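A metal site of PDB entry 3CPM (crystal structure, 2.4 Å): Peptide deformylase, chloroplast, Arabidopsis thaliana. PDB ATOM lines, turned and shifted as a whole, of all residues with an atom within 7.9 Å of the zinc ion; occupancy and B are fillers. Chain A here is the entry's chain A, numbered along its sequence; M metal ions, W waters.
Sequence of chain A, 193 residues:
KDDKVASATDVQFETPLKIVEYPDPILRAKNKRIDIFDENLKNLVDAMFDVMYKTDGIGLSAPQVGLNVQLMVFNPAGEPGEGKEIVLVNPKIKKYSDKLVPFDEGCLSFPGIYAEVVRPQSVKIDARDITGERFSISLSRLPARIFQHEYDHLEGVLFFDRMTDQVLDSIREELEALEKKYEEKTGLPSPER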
ATOM      1  N   LEU A  27       4.324   5.292 -14.392  1.00  0.00           N
ATOM      2  CA  LEU A  27       4.254   3.990 -15.028  1.00  0.00           C
ATOM      3  C   LEU A  27       4.934   3.972 -16.389  1.00  0.00           C
ATOM      4  O   LEU A  27       5.067   2.908 -17.007  1.00  0.00           O
ATOM      5  CB  LEU A  27       2.803   3.542 -15.146  1.00  0.00           C
ATOM      6  CG  LEU A  27       2.117   3.521 -13.768  1.00  0.00           C
ATOM      7  CD1 LEU A  27       0.676   3.097 -13.941  1.00  0.00           C
ATOM      8  CD2 LEU A  27       2.859   2.594 -12.819  1.00  0.00           C
ATOM      9  N   GLY A  59       1.544 -10.143  -8.749  1.00  0.00           N
ATOM     10  CA  GLY A  59       2.835  -9.622  -9.151  1.00  0.00           C
ATOM     11  C   GLY A  59       2.828  -8.112  -8.960  1.00  0.00           C
ATOM     12  O   GLY A  59       1.772  -7.477  -8.952  1.00  0.00           O
ATOM     13  N   LEU A  60       4.010  -7.537  -8.799  1.00  0.00           N
ATOM     14  CA  LEU A  60       4.108  -6.103  -8.597  1.00  0.00           C
ATOM     15  C   LEU A  60       5.504  -5.617  -8.931  1.00  0.00           C
ATOM     16  O   LEU A  60       6.498  -6.238  -8.566  1.00  0.00           O
ATOM     17  CB  LEU A  60       3.757  -5.763  -7.139  1.00  0.00           C
ATOM     18  CG  LEU A  60       3.702  -4.291  -6.726  1.00  0.00           C
ATOM     19  CD1 LEU A  60       2.483  -3.619  -7.360  1.00  0.00           C
ATOM     20  CD2 LEU A  60       3.611  -4.211  -5.204  1.00  0.00           C
ATOM     21  N   SER A  61       5.588  -4.490  -9.637  1.00  0.00           N
ATOM     22  CA  SER A  61       6.866  -3.905  -9.996  1.00  0.00           C
ATOM     23  C   SER A  61       6.974  -2.578  -9.260  1.00  0.00           C
ATOM     24  O   SER A  61       5.967  -1.931  -8.996  1.00  0.00           O
ATOM     25  CB  SER A  61       6.935  -3.693 -11.499  1.00  0.00           C
ATOM     26  OG  SER A  61       5.937  -2.782 -11.920  1.00  0.00           O
ATOM     27  N   GLN A  64       5.009   0.597  -9.881  1.00  0.00           N
ATOM     28  CA  GLN A  64       3.654   0.544  -9.354  1.00  0.00           C
ATOM     29  C   GLN A  64       3.502   1.011  -7.911  1.00  0.00           C
ATOM     30  O   GLN A  64       2.394   1.137  -7.406  1.00  0.00           O
ATOM     31  CB  GLN A  64       3.087  -0.863  -9.504  1.00  0.00           C
ATOM     32  CG  GLN A  64       2.584  -1.162 -10.901  1.00  0.00           C
ATOM     33  CD  GLN A  64       2.118  -2.591 -11.053  1.00  0.00           C
ATOM     34  OE1 GLN A  64       2.927  -3.521 -10.994  1.00  0.00           O
ATOM     35  NE2 GLN A  64       0.812  -2.778 -11.246  1.00  0.00           N
ATOM     36  N   GLU A 105      -5.251 -11.077 -18.684  1.00  0.00           N
ATOM     37  CA  GLU A 105      -4.404 -10.483 -17.658  1.00  0.00           C
ATOM     38  C   GLU A 105      -5.060  -9.356 -16.892  1.00  0.00           C
ATOM     39  O   GLU A 105      -5.865  -8.594 -17.428  1.00  0.00           O
ATOM     40  CB  GLU A 105      -3.127  -9.936 -18.286  1.00  0.00           C
ATOM     41  CG  GLU A 105      -2.191 -10.988 -18.858  1.00  0.00           C
ATOM     42  CD  GLU A 105      -1.000 -10.361 -19.566  1.00  0.00           C
ATOM     43  OE1 GLU A 105      -0.477  -9.359 -19.033  1.00  0.00           O
ATOM     44  OE2 GLU A 105      -0.592 -10.872 -20.627  1.00  0.00           O
ATOM     45  N   GLY A 106      -4.720  -9.262 -15.617  1.00  0.00           N
ATOM     46  CA  GLY A 106      -5.218  -8.195 -14.776  1.00  0.00           C
ATOM     47  C   GLY A 106      -3.983  -7.398 -14.372  1.00  0.00           C
ATOM     48  O   GLY A 106      -2.852  -7.842 -14.617  1.00  0.00           O
ATOM     49  N   CYS A 107      -4.194  -6.227 -13.779  1.00  0.00           N
ATOM     50  CA  CYS A 107      -3.093  -5.379 -13.326  1.00  0.00           C
ATOM     51  C   CYS A 107      -3.605  -4.505 -12.195  1.00  0.00           C
ATOM     52  O   CYS A 107      -4.707  -3.961 -12.274  1.00  0.00           O
ATOM     53  CB  CYS A 107      -2.559  -4.513 -14.472  1.00  0.00           C
ATOM     54  SG  CYS A 107      -1.194  -3.407 -14.002  1.00  0.00           S
ATOM     55  N   LEU A 108      -2.791  -4.371 -11.157  1.00  0.00           N
ATOM     56  CA  LEU A 108      -3.143  -3.564  -9.995  1.00  0.00           C
ATOM     57  C   LEU A 108      -3.290  -2.080 -10.330  1.00  0.00           C
ATOM     58  O   LEU A 108      -3.946  -1.342  -9.598  1.00  0.00           O
ATOM     59  CB  LEU A 108      -2.088  -3.755  -8.893  1.00  0.00           C
ATOM     60  CG  LEU A 108      -2.284  -4.880  -7.859  1.00  0.00           C
ATOM     61  CD1 LEU A 108      -3.367  -5.841  -8.284  1.00  0.00           C
ATOM     62  CD2 LEU A 108      -0.963  -5.601  -7.655  1.00  0.00           C
ATOM     63  N   SER A 109      -2.700  -1.654 -11.434  1.00  0.00           N
ATOM     64  CA  SER A 109      -2.795  -0.254 -11.831  1.00  0.00           C
ATOM     65  C   SER A 109      -4.022   0.008 -12.704  1.00  0.00           C
ATOM     66  O   SER A 109      -4.247   1.126 -13.163  1.00  0.00           O
ATOM     67  CB  SER A 109      -1.538   0.170 -12.580  1.00  0.00           C
ATOM     68  OG  SER A 109      -0.401   0.095 -11.736  1.00  0.00           O
ATOM     69  N   PHE A 110      -4.803  -1.044 -12.933  1.00  0.00           N
ATOM     70  CA  PHE A 110      -6.025  -0.966 -13.738  1.00  0.00           C
ATOM     71  C   PHE A 110      -7.101  -1.748 -12.978  1.00  0.00           C
ATOM     72  O   PHE A 110      -7.528  -2.832 -13.383  1.00  0.00           O
ATOM     73  CB  PHE A 110      -5.796  -1.620 -15.112  1.00  0.00           C
ATOM     74  CG  PHE A 110      -4.790  -0.875 -15.983  1.00  0.00           C
ATOM     75  CD1 PHE A 110      -5.228  -0.022 -16.996  1.00  0.00           C
ATOM     76  CD2 PHE A 110      -3.430  -1.068 -15.802  1.00  0.00           C
ATOM     77  CE1 PHE A 110      -4.314   0.630 -17.822  1.00  0.00           C
ATOM     78  CE2 PHE A 110      -2.497  -0.416 -16.631  1.00  0.00           C
ATOM     79  CZ  PHE A 110      -2.954   0.437 -17.641  1.00  0.00           C
ATOM     80  N   ARG A 119       1.335 -13.814 -25.263  1.00  0.00           N
ATOM     81  CA  ARG A 119       2.769 -13.737 -24.990  1.00  0.00           C
ATOM     82  C   ARG A 119       3.440 -15.099 -25.157  1.00  0.00           C
ATOM     83  O   ARG A 119       2.769 -16.138 -25.179  1.00  0.00           O
ATOM     84  CB  ARG A 119       3.034 -13.298 -23.552  1.00  0.00           C
ATOM     85  CG  ARG A 119       2.404 -12.007 -23.069  1.00  0.00           C
ATOM     86  CD  ARG A 119       2.808 -11.803 -21.611  1.00  0.00           C
ATOM     87  NE  ARG A 119       2.140 -10.684 -20.962  1.00  0.00           N
ATOM     88  CZ  ARG A 119       2.550  -9.426 -21.012  1.00  0.00           C
ATOM     89  NH1 ARG A 119       3.636  -9.109 -21.704  1.00  0.00           N
ATOM     90  NH2 ARG A 119       1.861  -8.483 -20.383  1.00  0.00           N
ATOM     91  N   ILE A 146       3.328 -14.032 -15.465  1.00  0.00           N
ATOM     92  CA  ILE A 146       3.398 -12.921 -14.519  1.00  0.00           C
ATOM     93  C   ILE A 146       4.712 -12.176 -14.725  1.00  0.00           C
ATOM     94  O   ILE A 146       4.749 -10.946 -14.702  1.00  0.00           O
ATOM     95  CB  ILE A 146       3.327 -13.436 -13.048  1.00  0.00           C
ATOM     96  CG1 ILE A 146       1.959 -14.094 -12.795  1.00  0.00           C
ATOM     97  CG2 ILE A 146       3.556 -12.291 -12.069  1.00  0.00           C
ATOM     98  CD1 ILE A 146       1.847 -14.773 -11.448  1.00  0.00           C
ATOM     99  N   HIS A 149       4.669  -9.755 -17.843  1.00  0.00           N
ATOM    100  CA  HIS A 149       3.788  -8.617 -17.567  1.00  0.00           C
ATOM    101  C   HIS A 149       4.555  -7.603 -16.713  1.00  0.00           C
ATOM    102  O   HIS A 149       4.517  -6.399 -16.981  1.00  0.00           O
ATOM    103  CB  HIS A 149       2.542  -9.099 -16.816  1.00  0.00           C
ATOM    104  CG  HIS A 149       1.661  -7.976 -16.329  1.00  0.00           C
ATOM    105  ND1 HIS A 149       0.581  -7.520 -17.057  1.00  0.00           N
ATOM    106  CD2 HIS A 149       1.717  -7.217 -15.217  1.00  0.00           C
ATOM    107  CE1 HIS A 149       0.016  -6.510 -16.411  1.00  0.00           C
ATOM    108  NE2 HIS A 149       0.692  -6.303 -15.289  1.00  0.00           N
ATOM    109  N   GLU A 150       5.273  -8.096 -15.696  1.00  0.00           N
ATOM    110  CA  GLU A 150       6.040  -7.220 -14.794  1.00  0.00           C
ATOM    111  C   GLU A 150       7.328  -6.687 -15.428  1.00  0.00           C
ATOM    112  O   GLU A 150       7.781  -5.590 -15.099  1.00  0.00           O
ATOM    113  CB  GLU A 150       6.388  -7.950 -13.493  1.00  0.00           C
ATOM    114  CG  GLU A 150       5.216  -8.488 -12.678  1.00  0.00           C
ATOM    115  CD  GLU A 150       4.157  -7.438 -12.332  1.00  0.00           C
ATOM    116  OE1 GLU A 150       4.499  -6.238 -12.205  1.00  0.00           O
ATOM    117  OE2 GLU A 150       2.982  -7.825 -12.169  1.00  0.00           O
ATOM    118  N   ASP A 152       7.613  -5.869 -18.442  1.00  0.00           N
ATOM    119  CA  ASP A 152       7.156  -4.754 -19.267  1.00  0.00           C
ATOM    120  C   ASP A 152       7.050  -3.491 -18.436  1.00  0.00           C
ATOM    121  O   ASP A 152       7.426  -2.405 -18.891  1.00  0.00           O
ATOM    122  CB  ASP A 152       5.801  -5.073 -19.891  1.00  0.00           C
ATOM    123  CG  ASP A 152       5.920  -5.879 -21.161  1.00  0.00           C
ATOM    124  OD1 ASP A 152       7.042  -6.087 -21.647  1.00  0.00           O
ATOM    125  OD2 ASP A 152       4.873  -6.308 -21.674  1.00  0.00           O
ATOM    126  N   HIS A 153       6.516  -3.629 -17.225  1.00  0.00           N
ATOM    127  CA  HIS A 153       6.385  -2.492 -16.324  1.00  0.00           C
ATOM    128  C   HIS A 153       7.746  -1.839 -16.176  1.00  0.00           C
ATOM    129  O   HIS A 153       7.878  -0.621 -16.136  1.00  0.00           O
ATOM    130  CB  HIS A 153       5.888  -2.933 -14.942  1.00  0.00           C
ATOM    131  CG  HIS A 153       4.405  -3.048 -14.832  1.00  0.00           C
ATOM    132  ND1 HIS A 153       3.548  -2.001 -15.139  1.00  0.00           N
ATOM    133  CD2 HIS A 153       3.613  -4.061 -14.416  1.00  0.00           C
ATOM    134  CE1 HIS A 153       2.304  -2.378 -14.910  1.00  0.00           C
ATOM    135  NE2 HIS A 153       2.311  -3.623 -14.484  1.00  0.00           N
ATOM    136  N   VAL A 157       6.356  -0.209 -20.128  1.00  0.00           N
ATOM    137  CA  VAL A 157       5.345  -0.784 -21.003  1.00  0.00           C
ATOM    138  C   VAL A 157       4.135  -1.320 -20.231  1.00  0.00           C
ATOM    139  O   VAL A 157       4.280  -2.117 -19.305  1.00  0.00           O
ATOM    140  CB  VAL A 157       5.944  -1.930 -21.856  1.00  0.00           C
ATOM    141  CG1 VAL A 157       4.857  -2.587 -22.708  1.00  0.00           C
ATOM    142  CG2 VAL A 157       7.076  -1.397 -22.722  1.00  0.00           C
ATOM    143  N   LEU A 158       2.944  -0.885 -20.628  1.00  0.00           N
ATOM    144  CA  LEU A 158       1.708  -1.319 -19.986  1.00  0.00           C
ATOM    145  C   LEU A 158       1.022  -2.414 -20.797  1.00  0.00           C
ATOM    146  O   LEU A 158       1.094  -2.407 -22.030  1.00  0.00           O
ATOM    147  CB  LEU A 158       0.777  -0.112 -19.812  1.00  0.00           C
ATOM    148  CG  LEU A 158       0.905   0.628 -18.476  1.00  0.00           C
ATOM    149  CD1 LEU A 158       2.330   0.538 -17.946  1.00  0.00           C
ATOM    150  CD2 LEU A 158       0.464   2.081 -18.651  1.00  0.00           C
ATOM    151  N   PHE A 159       0.349  -3.339 -20.117  1.00  0.00           N
ATOM    152  CA  PHE A 159      -0.289  -4.474 -20.783  1.00  0.00           C
ATOM    153  C   PHE A 159      -1.241  -4.185 -21.924  1.00  0.00           C
ATOM    154  O   PHE A 159      -1.352  -5.005 -22.846  1.00  0.00           O
ATOM    155  CB  PHE A 159      -0.936  -5.425 -19.755  1.00  0.00           C
ATOM    156  CG  PHE A 159      -2.274  -4.973 -19.206  1.00  0.00           C
ATOM    157  CD1 PHE A 159      -2.538  -3.629 -18.938  1.00  0.00           C
ATOM    158  CD2 PHE A 159      -3.260  -5.914 -18.894  1.00  0.00           C
ATOM    159  CE1 PHE A 159      -3.759  -3.241 -18.364  1.00  0.00           C
ATOM    160  CE2 PHE A 159      -4.478  -5.542 -18.309  1.00  0.00           C
ATOM    161  CZ  PHE A 159      -4.723  -4.198 -18.044  1.00  0.00           C
HETATM  162 ZN    ZN M   1       0.787  -4.706 -13.962  1.00  0.00          ZN
HETATM  163  O   HOH W   1       1.537  -5.814 -12.228  1.00  0.00           O
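A ring nitrogen (ND1) of His 149 sits at hydrogen-bond distance from the side-chain carboxylate of Glu 105 (2.9 Å). OE1 of Gln 64 sits close to OE1 of Glu 150 (3.4 Å). The side-chain amide nitrogen (NE2) of Gln 64 lies within hydrogen-bond range of the side-chain hydroxyl (OG) of Ser 109 (3.2 Å). The backbone NH (N) of Ser 109 lies close to the side-chain sulfur (SG) of Cys 107, at 3.5 Å. The side-chain amide oxygen (OE1) of Gln 64 sits at hydrogen-bond distance from the backbone NH (N) of Ser 61, 3.1 Å away. The side-chain sulfur (SG) of Cys 107 lies close to the side-chain amide nitrogen (NE2) of Gln 64, 3.5 Å away.
Gln 64 touches the zinc ion. Of the 20 residues printed, 4 come within 4 Å of the zinc ion.
The zinc ion is bound by NE2 of His 153 (1.9 Å). The zinc ion is bound by NE2 of His 149 (2.1 Å). Water W1 is bound to the zinc ion (2.2 Å). The side-chain sulfur (SG) of Cys 107 is bound to the zinc ion, at 2.4 Å. The zinc ion has four donor atoms within binding distance.
Water W1 lies within hydrogen-bond range of the side-chain carboxylate (OE2) of Glu 150 (2.5 Å) and the side-chain amide oxygen (OE1) of Gln 64 (3.0 Å).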
